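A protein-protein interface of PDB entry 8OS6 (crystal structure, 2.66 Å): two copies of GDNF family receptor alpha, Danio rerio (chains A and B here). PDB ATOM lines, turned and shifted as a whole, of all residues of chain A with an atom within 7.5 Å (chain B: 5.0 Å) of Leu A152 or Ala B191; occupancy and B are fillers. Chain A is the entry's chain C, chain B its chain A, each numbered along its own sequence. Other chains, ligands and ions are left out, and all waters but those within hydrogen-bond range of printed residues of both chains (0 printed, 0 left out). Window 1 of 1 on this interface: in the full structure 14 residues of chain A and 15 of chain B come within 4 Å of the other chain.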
ATOM      1  N   PRO A 149      25.215  10.041 -14.436  1.00  0.00           N
ATOM      2  CA  PRO A 149      24.655  10.770 -15.579  1.00  0.00           C
ATOM      3  C   PRO A 149      25.428  10.507 -16.866  1.00  0.00           C
ATOM      4  O   PRO A 149      26.484   9.875 -16.879  1.00  0.00           O
ATOM      5  CB  PRO A 149      24.782  12.235 -15.150  1.00  0.00           C
ATOM      6  CG  PRO A 149      26.007  12.248 -14.293  1.00  0.00           C
ATOM      7  CD  PRO A 149      26.026  10.920 -13.570  1.00  0.00           C
ATOM      8  N   ASN A 150      24.869  11.013 -17.964  1.00  0.00           N
ATOM      9  CA  ASN A 150      25.558  11.037 -19.247  1.00  0.00           C
ATOM     10  C   ASN A 150      26.397  12.305 -19.333  1.00  0.00           C
ATOM     11  O   ASN A 150      25.986  13.368 -18.858  1.00  0.00           O
ATOM     12  CB  ASN A 150      24.563  10.982 -20.406  1.00  0.00           C
ATOM     13  CG  ASN A 150      25.245  10.806 -21.754  1.00  0.00           C
ATOM     14  OD1 ASN A 150      25.473  11.775 -22.479  1.00  0.00           O
ATOM     15  ND2 ASN A 150      25.576   9.564 -22.094  1.00  0.00           N
ATOM     16  N   CYS A 151      27.575  12.191 -19.950  1.00  0.00           N
ATOM     17  CA  CYS A 151      28.527  13.295 -19.915  1.00  0.00           C
ATOM     18  C   CYS A 151      28.026  14.525 -20.660  1.00  0.00           C
ATOM     19  O   CYS A 151      28.533  15.625 -20.418  1.00  0.00           O
ATOM     20  CB  CYS A 151      29.875  12.849 -20.484  1.00  0.00           C
ATOM     21  SG  CYS A 151      30.604  11.415 -19.636  1.00  0.00           S
ATOM     22  N   LEU A 152      27.045  14.383 -21.554  1.00  0.00           N
ATOM     23  CA  LEU A 152      26.464  15.571 -22.171  1.00  0.00           C
ATOM     24  C   LEU A 152      25.581  16.314 -21.177  1.00  0.00           C
ATOM     25  O   LEU A 152      25.658  17.542 -21.059  1.00  0.00           O
ATOM     26  CB  LEU A 152      25.669  15.200 -23.422  1.00  0.00           C
ATOM     27  CG  LEU A 152      25.001  16.387 -24.128  1.00  0.00           C
ATOM     28  CD1 LEU A 152      26.025  17.441 -24.535  1.00  0.00           C
ATOM     29  CD2 LEU A 152      24.208  15.925 -25.342  1.00  0.00           C
ATOM     30  N   THR A 153      24.735  15.583 -20.448  1.00  0.00           N
ATOM     31  CA  THR A 153      23.887  16.226 -19.451  1.00  0.00           C
ATOM     32  C   THR A 153      24.728  16.893 -18.371  1.00  0.00           C
ATOM     33  O   THR A 153      24.411  18.000 -17.920  1.00  0.00           O
ATOM     34  CB  THR A 153      22.933  15.206 -18.829  1.00  0.00           C
ATOM     35  OG1 THR A 153      23.688  14.173 -18.184  1.00  0.00           O
ATOM     36  CG2 THR A 153      22.041  14.586 -19.895  1.00  0.00           C
ATOM     37  N   LEU A 154      25.814  16.239 -17.950  1.00  0.00           N
ATOM     38  CA  LEU A 154      26.650  16.803 -16.896  1.00  0.00           C
ATOM     39  C   LEU A 154      27.340  18.081 -17.362  1.00  0.00           C
ATOM     40  O   LEU A 154      27.476  19.035 -16.587  1.00  0.00           O
ATOM     41  CB  LEU A 154      27.678  15.770 -16.438  1.00  0.00           C
ATOM     42  CG  LEU A 154      28.424  16.093 -15.143  1.00  0.00           C
ATOM     43  CD1 LEU A 154      27.482  16.026 -13.953  1.00  0.00           C
ATOM     44  CD2 LEU A 154      29.597  15.152 -14.941  1.00  0.00           C
ATOM     45  N   GLN A 155      27.777  18.123 -18.624  1.00  0.00           N
ATOM     46  CA  GLN A 155      28.376  19.345 -19.154  1.00  0.00           C
ATOM     47  C   GLN A 155      27.374  20.493 -19.153  1.00  0.00           C
ATOM     48  O   GLN A 155      27.743  21.650 -18.915  1.00  0.00           O
ATOM     49  CB  GLN A 155      28.902  19.112 -20.570  1.00  0.00           C
ATOM     50  CG  GLN A 155      30.274  18.471 -20.636  1.00  0.00           C
ATOM     51  CD  GLN A 155      30.835  18.454 -22.044  1.00  0.00           C
ATOM     52  OE1 GLN A 155      30.968  17.395 -22.660  1.00  0.00           O
ATOM     53  NE2 GLN A 155      31.170  19.631 -22.563  1.00  0.00           N
ATOM     54  N   VAL A 156      26.105  20.197 -19.435  1.00  0.00           N
ATOM     55  CA  VAL A 156      25.088  21.242 -19.421  1.00  0.00           C
ATOM     56  C   VAL A 156      24.821  21.706 -17.998  1.00  0.00           C
ATOM     57  O   VAL A 156      24.543  22.889 -17.763  1.00  0.00           O
ATOM     58  CB  VAL A 156      23.800  20.739 -20.096  1.00  0.00           C
ATOM     59  CG1 VAL A 156      22.692  21.765 -19.948  1.00  0.00           C
ATOM     60  CG2 VAL A 156      24.056  20.430 -21.561  1.00  0.00           C
ATOM     61  N   SER A 157      24.901  20.794 -17.029  1.00  0.00           N
ATOM     62  CA  SER A 157      24.695  21.166 -15.635  1.00  0.00           C
ATOM     63  C   SER A 157      25.785  22.118 -15.156  1.00  0.00           C
ATOM     64  O   SER A 157      25.500  23.127 -14.501  1.00  0.00           O
ATOM     65  CB  SER A 157      24.653  19.910 -14.767  1.00  0.00           C
ATOM     66  OG  SER A 157      24.409  20.236 -13.412  1.00  0.00           O
ATOM     67  N   CYS A 158      27.044  21.812 -15.477  1.00  0.00           N
ATOM     68  CA  CYS A 158      28.147  22.656 -15.025  1.00  0.00           C
ATOM     69  C   CYS A 158      28.126  24.014 -15.713  1.00  0.00           C
ATOM     70  O   CYS A 158      28.476  25.031 -15.104  1.00  0.00           O
ATOM     71  CB  CYS A 158      29.480  21.954 -15.279  1.00  0.00           C
ATOM     72  SG  CYS A 158      30.959  22.963 -14.979  1.00  0.00           S
ATOM     73  N   LYS A 159      27.721  24.055 -16.981  1.00  0.00           N
ATOM     74  CA  LYS A 159      27.781  25.303 -17.731  1.00  0.00           C
ATOM     75  C   LYS A 159      26.687  26.281 -17.325  1.00  0.00           C
ATOM     76  O   LYS A 159      26.825  27.481 -17.584  1.00  0.00           O
ATOM     77  CB  LYS A 159      27.708  25.003 -19.229  1.00  0.00           C
ATOM     78  CG  LYS A 159      28.944  24.296 -19.766  1.00  0.00           C
ATOM     79  CD  LYS A 159      28.686  23.674 -21.127  1.00  0.00           C
ATOM     80  CE  LYS A 159      29.937  23.009 -21.682  1.00  0.00           C
ATOM     81  NZ  LYS A 159      31.062  23.974 -21.835  1.00  0.00           N
ATOM     82  N   CYS A 221      30.686  10.613 -14.752  1.00  0.00           N
ATOM     83  CA  CYS A 221      29.857  10.635 -15.950  1.00  0.00           C
ATOM     84  C   CYS A 221      30.258   9.467 -16.842  1.00  0.00           C
ATOM     85  O   CYS A 221      31.373   8.949 -16.754  1.00  0.00           O
ATOM     86  CB  CYS A 221      29.974  11.973 -16.698  1.00  0.00           C
ATOM     87  SG  CYS A 221      31.341  12.130 -17.874  1.00  0.00           S
ATOM     88  N   ASP A 222      29.324   9.053 -17.699  1.00  0.00           N
ATOM     89  CA  ASP A 222      29.495   7.884 -18.554  1.00  0.00           C
ATOM     90  C   ASP A 222      29.006   8.211 -19.960  1.00  0.00           C
ATOM     91  O   ASP A 222      28.182   9.108 -20.158  1.00  0.00           O
ATOM     92  CB  ASP A 222      28.751   6.671 -17.968  1.00  0.00           C
ATOM     93  CG  ASP A 222      28.284   5.698 -19.028  1.00  0.00           C
ATOM     94  OD1 ASP A 222      29.135   5.177 -19.782  1.00  0.00           O
ATOM     95  OD2 ASP A 222      27.062   5.451 -19.103  1.00  0.00           O
ATOM     96  N   CYS A 223      29.540   7.471 -20.939  1.00  0.00           N
ATOM     97  CA  CYS A 223      29.313   7.752 -22.353  1.00  0.00           C
ATOM     98  C   CYS A 223      28.559   6.625 -23.051  1.00  0.00           C
ATOM     99  O   CYS A 223      28.930   6.205 -24.153  1.00  0.00           O
ATOM    100  CB  CYS A 223      30.651   7.993 -23.063  1.00  0.00           C
ATOM    101  SG  CYS A 223      31.387   9.605 -22.741  1.00  0.00           S
ATOM    102  N   SER A 225      25.850   6.532 -24.831  1.00  0.00           N
ATOM    103  CA  SER A 225      24.889   7.297 -25.614  1.00  0.00           C
ATOM    104  C   SER A 225      24.514   6.626 -26.931  1.00  0.00           C
ATOM    105  O   SER A 225      23.623   7.123 -27.628  1.00  0.00           O
ATOM    106  CB  SER A 225      25.437   8.706 -25.883  1.00  0.00           C
ATOM    107  OG  SER A 225      25.540   8.976 -27.269  1.00  0.00           O
ATOM    108  N   SER A 229      26.176  11.202 -30.054  1.00  0.00           N
ATOM    109  CA  SER A 229      27.115  11.928 -29.207  1.00  0.00           C
ATOM    110  C   SER A 229      27.956  10.908 -28.433  1.00  0.00           C
ATOM    111  O   SER A 229      27.859  10.776 -27.213  1.00  0.00           O
ATOM    112  CB  SER A 229      26.392  12.887 -28.258  1.00  0.00           C
ATOM    113  OG  SER A 229      27.310  13.555 -27.409  1.00  0.00           O
ATOM    114  N   GLU A 232      32.212  12.943 -29.439  1.00  0.00           N
ATOM    115  CA  GLU A 232      32.421  14.084 -28.552  1.00  0.00           C
ATOM    116  C   GLU A 232      32.462  13.640 -27.097  1.00  0.00           C
ATOM    117  O   GLU A 232      33.210  14.198 -26.288  1.00  0.00           O
ATOM    118  CB  GLU A 232      31.319  15.125 -28.758  1.00  0.00           C
ATOM    119  CG  GLU A 232      31.398  16.309 -27.799  1.00  0.00           C
ATOM    120  CD  GLU A 232      30.282  17.316 -28.009  1.00  0.00           C
ATOM    121  OE1 GLU A 232      29.882  17.537 -29.172  1.00  0.00           O
ATOM    122  OE2 GLU A 232      29.801  17.884 -27.007  1.00  0.00           O
ATOM    123  N   CYS A 233      31.659  12.633 -26.748  1.00  0.00           N
ATOM    124  CA  CYS A 233      31.645  12.145 -25.375  1.00  0.00           C
ATOM    125  C   CYS A 233      32.970  11.488 -25.013  1.00  0.00           C
ATOM    126  O   CYS A 233      33.521  11.740 -23.935  1.00  0.00           O
ATOM    127  CB  CYS A 233      30.489  11.165 -25.186  1.00  0.00           C
ATOM    128  SG  CYS A 233      30.014  10.914 -23.468  1.00  0.00           S
ATOM    129  N   PHE A 236      35.771  13.900 -24.510  1.00  0.00           N
ATOM    130  CA  PHE A 236      35.671  14.596 -23.231  1.00  0.00           C
ATOM    131  C   PHE A 236      36.266  13.758 -22.104  1.00  0.00           C
ATOM    132  O   PHE A 236      37.186  14.196 -21.405  1.00  0.00           O
ATOM    133  CB  PHE A 236      34.205  14.933 -22.950  1.00  0.00           C
ATOM    134  CG  PHE A 236      33.964  15.531 -21.597  1.00  0.00           C
ATOM    135  CD1 PHE A 236      34.193  16.876 -21.371  1.00  0.00           C
ATOM    136  CD2 PHE A 236      33.494  14.751 -20.555  1.00  0.00           C
ATOM    137  CE1 PHE A 236      33.970  17.431 -20.130  1.00  0.00           C
ATOM    138  CE2 PHE A 236      33.268  15.300 -19.311  1.00  0.00           C
ATOM    139  CZ  PHE A 236      33.506  16.642 -19.098  1.00  0.00           C
ATOM    140  N   ASN B 189      31.007  21.775 -29.751  1.00  0.00           N
ATOM    141  CA  ASN B 189      30.497  21.496 -28.411  1.00  0.00           C
ATOM    142  C   ASN B 189      28.979  21.585 -28.465  1.00  0.00           C
ATOM    143  O   ASN B 189      28.427  22.675 -28.640  1.00  0.00           O
ATOM    144  CB  ASN B 189      31.064  22.461 -27.371  1.00  0.00           C
ATOM    145  CG  ASN B 189      30.777  22.013 -25.947  1.00  0.00           C
ATOM    146  OD1 ASN B 189      29.771  21.353 -25.685  1.00  0.00           O
ATOM    147  ND2 ASN B 189      31.665  22.364 -25.022  1.00  0.00           N
ATOM    148  N   TYR B 190      28.309  20.438 -28.323  1.00  0.00           N
ATOM    149  CA  TYR B 190      26.850  20.426 -28.313  1.00  0.00           C
ATOM    150  C   TYR B 190      26.299  21.162 -27.094  1.00  0.00           C
ATOM    151  O   TYR B 190      25.301  21.885 -27.196  1.00  0.00           O
ATOM    152  CB  TYR B 190      26.331  18.986 -28.332  1.00  0.00           C
ATOM    153  CG  TYR B 190      26.453  18.259 -29.658  1.00  0.00           C
ATOM    154  CD1 TYR B 190      26.351  18.937 -30.866  1.00  0.00           C
ATOM    155  CD2 TYR B 190      26.656  16.885 -29.696  1.00  0.00           C
ATOM    156  CE1 TYR B 190      26.457  18.268 -32.073  1.00  0.00           C
ATOM    157  CE2 TYR B 190      26.762  16.210 -30.898  1.00  0.00           C
ATOM    158  CZ  TYR B 190      26.662  16.906 -32.083  1.00  0.00           C
ATOM    159  OH  TYR B 190      26.767  16.233 -33.279  1.00  0.00           O
ATOM    160  N   ALA B 191      26.931  20.984 -25.931  1.00  0.00           N
ATOM    161  CA  ALA B 191      26.421  21.604 -24.712  1.00  0.00           C
ATOM    162  C   ALA B 191      26.381  23.121 -24.837  1.00  0.00           C
ATOM    163  O   ALA B 191      25.402  23.759 -24.431  1.00  0.00           O
ATOM    164  CB  ALA B 191      27.276  21.191 -23.514  1.00  0.00           C
ATOM    165  N   ASP B 192      27.434  23.722 -25.394  1.00  0.00           N
ATOM    166  CA  ASP B 192      27.460  25.171 -25.542  1.00  0.00           C
ATOM    167  C   ASP B 192      26.394  25.675 -26.504  1.00  0.00           C
ATOM    168  O   ASP B 192      26.006  26.844 -26.422  1.00  0.00           O
ATOM    169  CB  ASP B 192      28.837  25.631 -26.021  1.00  0.00           C
ATOM    170  CG  ASP B 192      29.919  25.407 -24.985  1.00  0.00           C
ATOM    171  OD1 ASP B 192      29.665  25.672 -23.790  1.00  0.00           O
ATOM    172  OD2 ASP B 192      31.022  24.961 -25.364  1.00  0.00           O
ATOM    173  N   CYS B 193      25.915  24.827 -27.417  1.00  0.00           N
ATOM    174  CA  CYS B 193      24.862  25.255 -28.331  1.00  0.00           C
ATOM    175  C   CYS B 193      23.493  25.156 -27.671  1.00  0.00           C
ATOM    176  O   CYS B 193      22.680  26.080 -27.784  1.00  0.00           O
ATOM    177  CB  CYS B 193      24.908  24.426 -29.620  1.00  0.00           C
ATOM    178  SG  CYS B 193      23.581  24.801 -30.805  1.00  0.00           S
ATOM    179  N   LEU B 194      23.230  24.057 -26.960  1.00  0.00           N
ATOM    180  CA  LEU B 194      21.929  23.888 -26.321  1.00  0.00           C
ATOM    181  C   LEU B 194      21.654  25.011 -25.328  1.00  0.00           C
ATOM    182  O   LEU B 194      20.552  25.571 -25.298  1.00  0.00           O
ATOM    183  CB  LEU B 194      21.853  22.529 -25.627  1.00  0.00           C
ATOM    184  CG  LEU B 194      21.635  21.316 -26.529  1.00  0.00           C
ATOM    185  CD1 LEU B 194      21.529  20.041 -25.704  1.00  0.00           C
ATOM    186  CD2 LEU B 194      20.393  21.501 -27.385  1.00  0.00           C
ATOM    187  N   LEU B 195      22.641  25.353 -24.497  1.00  0.00           N
ATOM    188  CA  LEU B 195      22.441  26.428 -23.531  1.00  0.00           C
ATOM    189  C   LEU B 195      22.105  27.736 -24.237  1.00  0.00           C
ATOM    190  O   LEU B 195      21.070  28.356 -23.967  1.00  0.00           O
ATOM    191  CB  LEU B 195      23.684  26.598 -22.656  1.00  0.00           C
ATOM    192  CG  LEU B 195      23.804  25.686 -21.437  1.00  0.00           C
ATOM    193  CD1 LEU B 195      25.035  26.074 -20.631  1.00  0.00           C
ATOM    194  CD2 LEU B 195      22.561  25.739 -20.565  1.00  0.00           C
ATOM    195  N   ALA B 249      22.481  18.597 -31.796  1.00  0.00           N
ATOM    196  CA  ALA B 249      22.569  18.750 -30.347  1.00  0.00           C
ATOM    197  C   ALA B 249      21.280  18.298 -29.672  1.00  0.00           C
ATOM    198  O   ALA B 249      21.306  17.540 -28.695  1.00  0.00           O
ATOM    199  CB  ALA B 249      22.884  20.202 -29.991  1.00  0.00           C
ATOM    200  N   ALA B 252      21.135  14.694 -29.683  1.00  0.00           N
ATOM    201  CA  ALA B 252      22.121  14.131 -28.767  1.00  0.00           C
ATOM    202  C   ALA B 252      21.590  14.107 -27.341  1.00  0.00           C
ATOM    203  O   ALA B 252      21.807  13.135 -26.607  1.00  0.00           O
ATOM    204  CB  ALA B 252      23.422  14.929 -28.842  1.00  0.00           C
ATOM    205  N   PHE B 253      20.882  15.163 -26.933  1.00  0.00           N
ATOM    206  CA  PHE B 253      20.398  15.235 -25.559  1.00  0.00           C
ATOM    207  C   PHE B 253      19.235  14.278 -25.328  1.00  0.00           C
ATOM    208  O   PHE B 253      19.161  13.624 -24.282  1.00  0.00           O
ATOM    209  CB  PHE B 253      19.977  16.663 -25.223  1.00  0.00           C
ATOM    210  CG  PHE B 253      19.896  16.932 -23.752  1.00  0.00           C
ATOM    211  CD1 PHE B 253      18.806  16.504 -23.013  1.00  0.00           C
ATOM    212  CD2 PHE B 253      20.916  17.607 -23.104  1.00  0.00           C
ATOM    213  CE1 PHE B 253      18.732  16.747 -21.654  1.00  0.00           C
ATOM    214  CE2 PHE B 253      20.849  17.853 -21.747  1.00  0.00           C
ATOM    215  CZ  PHE B 253      19.756  17.422 -21.020  1.00  0.00           C
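Printed residues of chain B within 4 Å of Leu A152: Ala B191 (3.9 Å), Ala B252 (3.7 Å) and Phe B253 (3.8 Å).
Of chain A, only Leu A152 (3.9 Å), Gln A155 (3.95 Å), Val A156 (3.8 Å) and Lys A159 (3.7 Å) come within 4 Å of Ala B191.
Of the printed residues of chain A, Asp B192 touches Lys A159 (2.9 Å).
Of the printed residues of chain A, Phe B253 touches Leu A152 (3.8 Å) and Thr A153 (3.8 Å).
Phe A236 touches none of the printed residues of chain B.
Cys A223 touches none of the printed residues of chain B.
The nearest residue of chain B that does not touch Leu A152 is Tyr B190 (4.1 Å).
OE2 of Glu A232 is in hydrogen-bond range of N of Tyr B190, at 3.2 Å.
NZ of Lys A159 lies within salt-bridge range of OD1 of Asp B192 (2.9 Å).
Ala B191 touches Leu A152 (N to CD1, 3.9 Å).
Leu A152 touches Ala B252 (CD2 to CB, 3.7 Å).
CZ of Phe B253 touches CG2 of Thr A153, at 3.8 Å.
NE2 of Gln A155 touches ND2 of Asn B189 (3.7 Å).
Val A156 touches Ala B191.
ND2 of Asn B189 touches NZ of Lys A159 (3.6 Å).
Lys A159 touches Ala B191 (CE to CB, 3.7 Å).
CD1 of Leu B195 touches CB of Lys A159 (3.2 Å).
CB of Ser A229 touches CB of Ala B252 (3.7 Å).
Asn B189 touches Glu A232 (OD1 to OE2, 3.7 Å).
The backbone NH (N) of Ala B191 lies within hydrogen-bond range of the side-chain amide oxygen (OD1) of Asn B189.
The side-chain amide nitrogen (ND2) of Asn B189 lies within hydrogen-bond range of the side-chain carboxylate (OD2) of Asp B192 (2.7 Å).
N of Leu A152 lies close to OD1 of Asn A150.
O of Asn A150 lies within hydrogen-bond range of OG1 of Thr A153 (2.5 Å).
The side-chain sulfur of Cys A151 is disulfide-bonded to the side-chain sulfur of Cys A221, at 2.0 Å.
SG of Cys A223 forms a disulfide with SG of Cys A233, 2.0 Å away.
Printed residues of chain B that touch a printed residue of chain A: Asn B189, Tyr B190, Ala B191, Asp B192, Leu B195, Ala B252 and Phe B253.
Hydrophobic or aromatic side chains of chain B that line the printed part of chain A: Tyr B190, Ala B191, Leu B195, Ala B252 and Phe B253.
Along chain B the printed residues that touch a printed residue of chain A span positions 189 to 253.
Among the printed residues, 14 pairs touch across the chains.
Among the printed residues, Asp or Glu carboxylates within 4 Å of a Lys or Arg side-chain nitrogen of the other chain: Lys A159 with Asp B192.
No position is printed for both chains.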
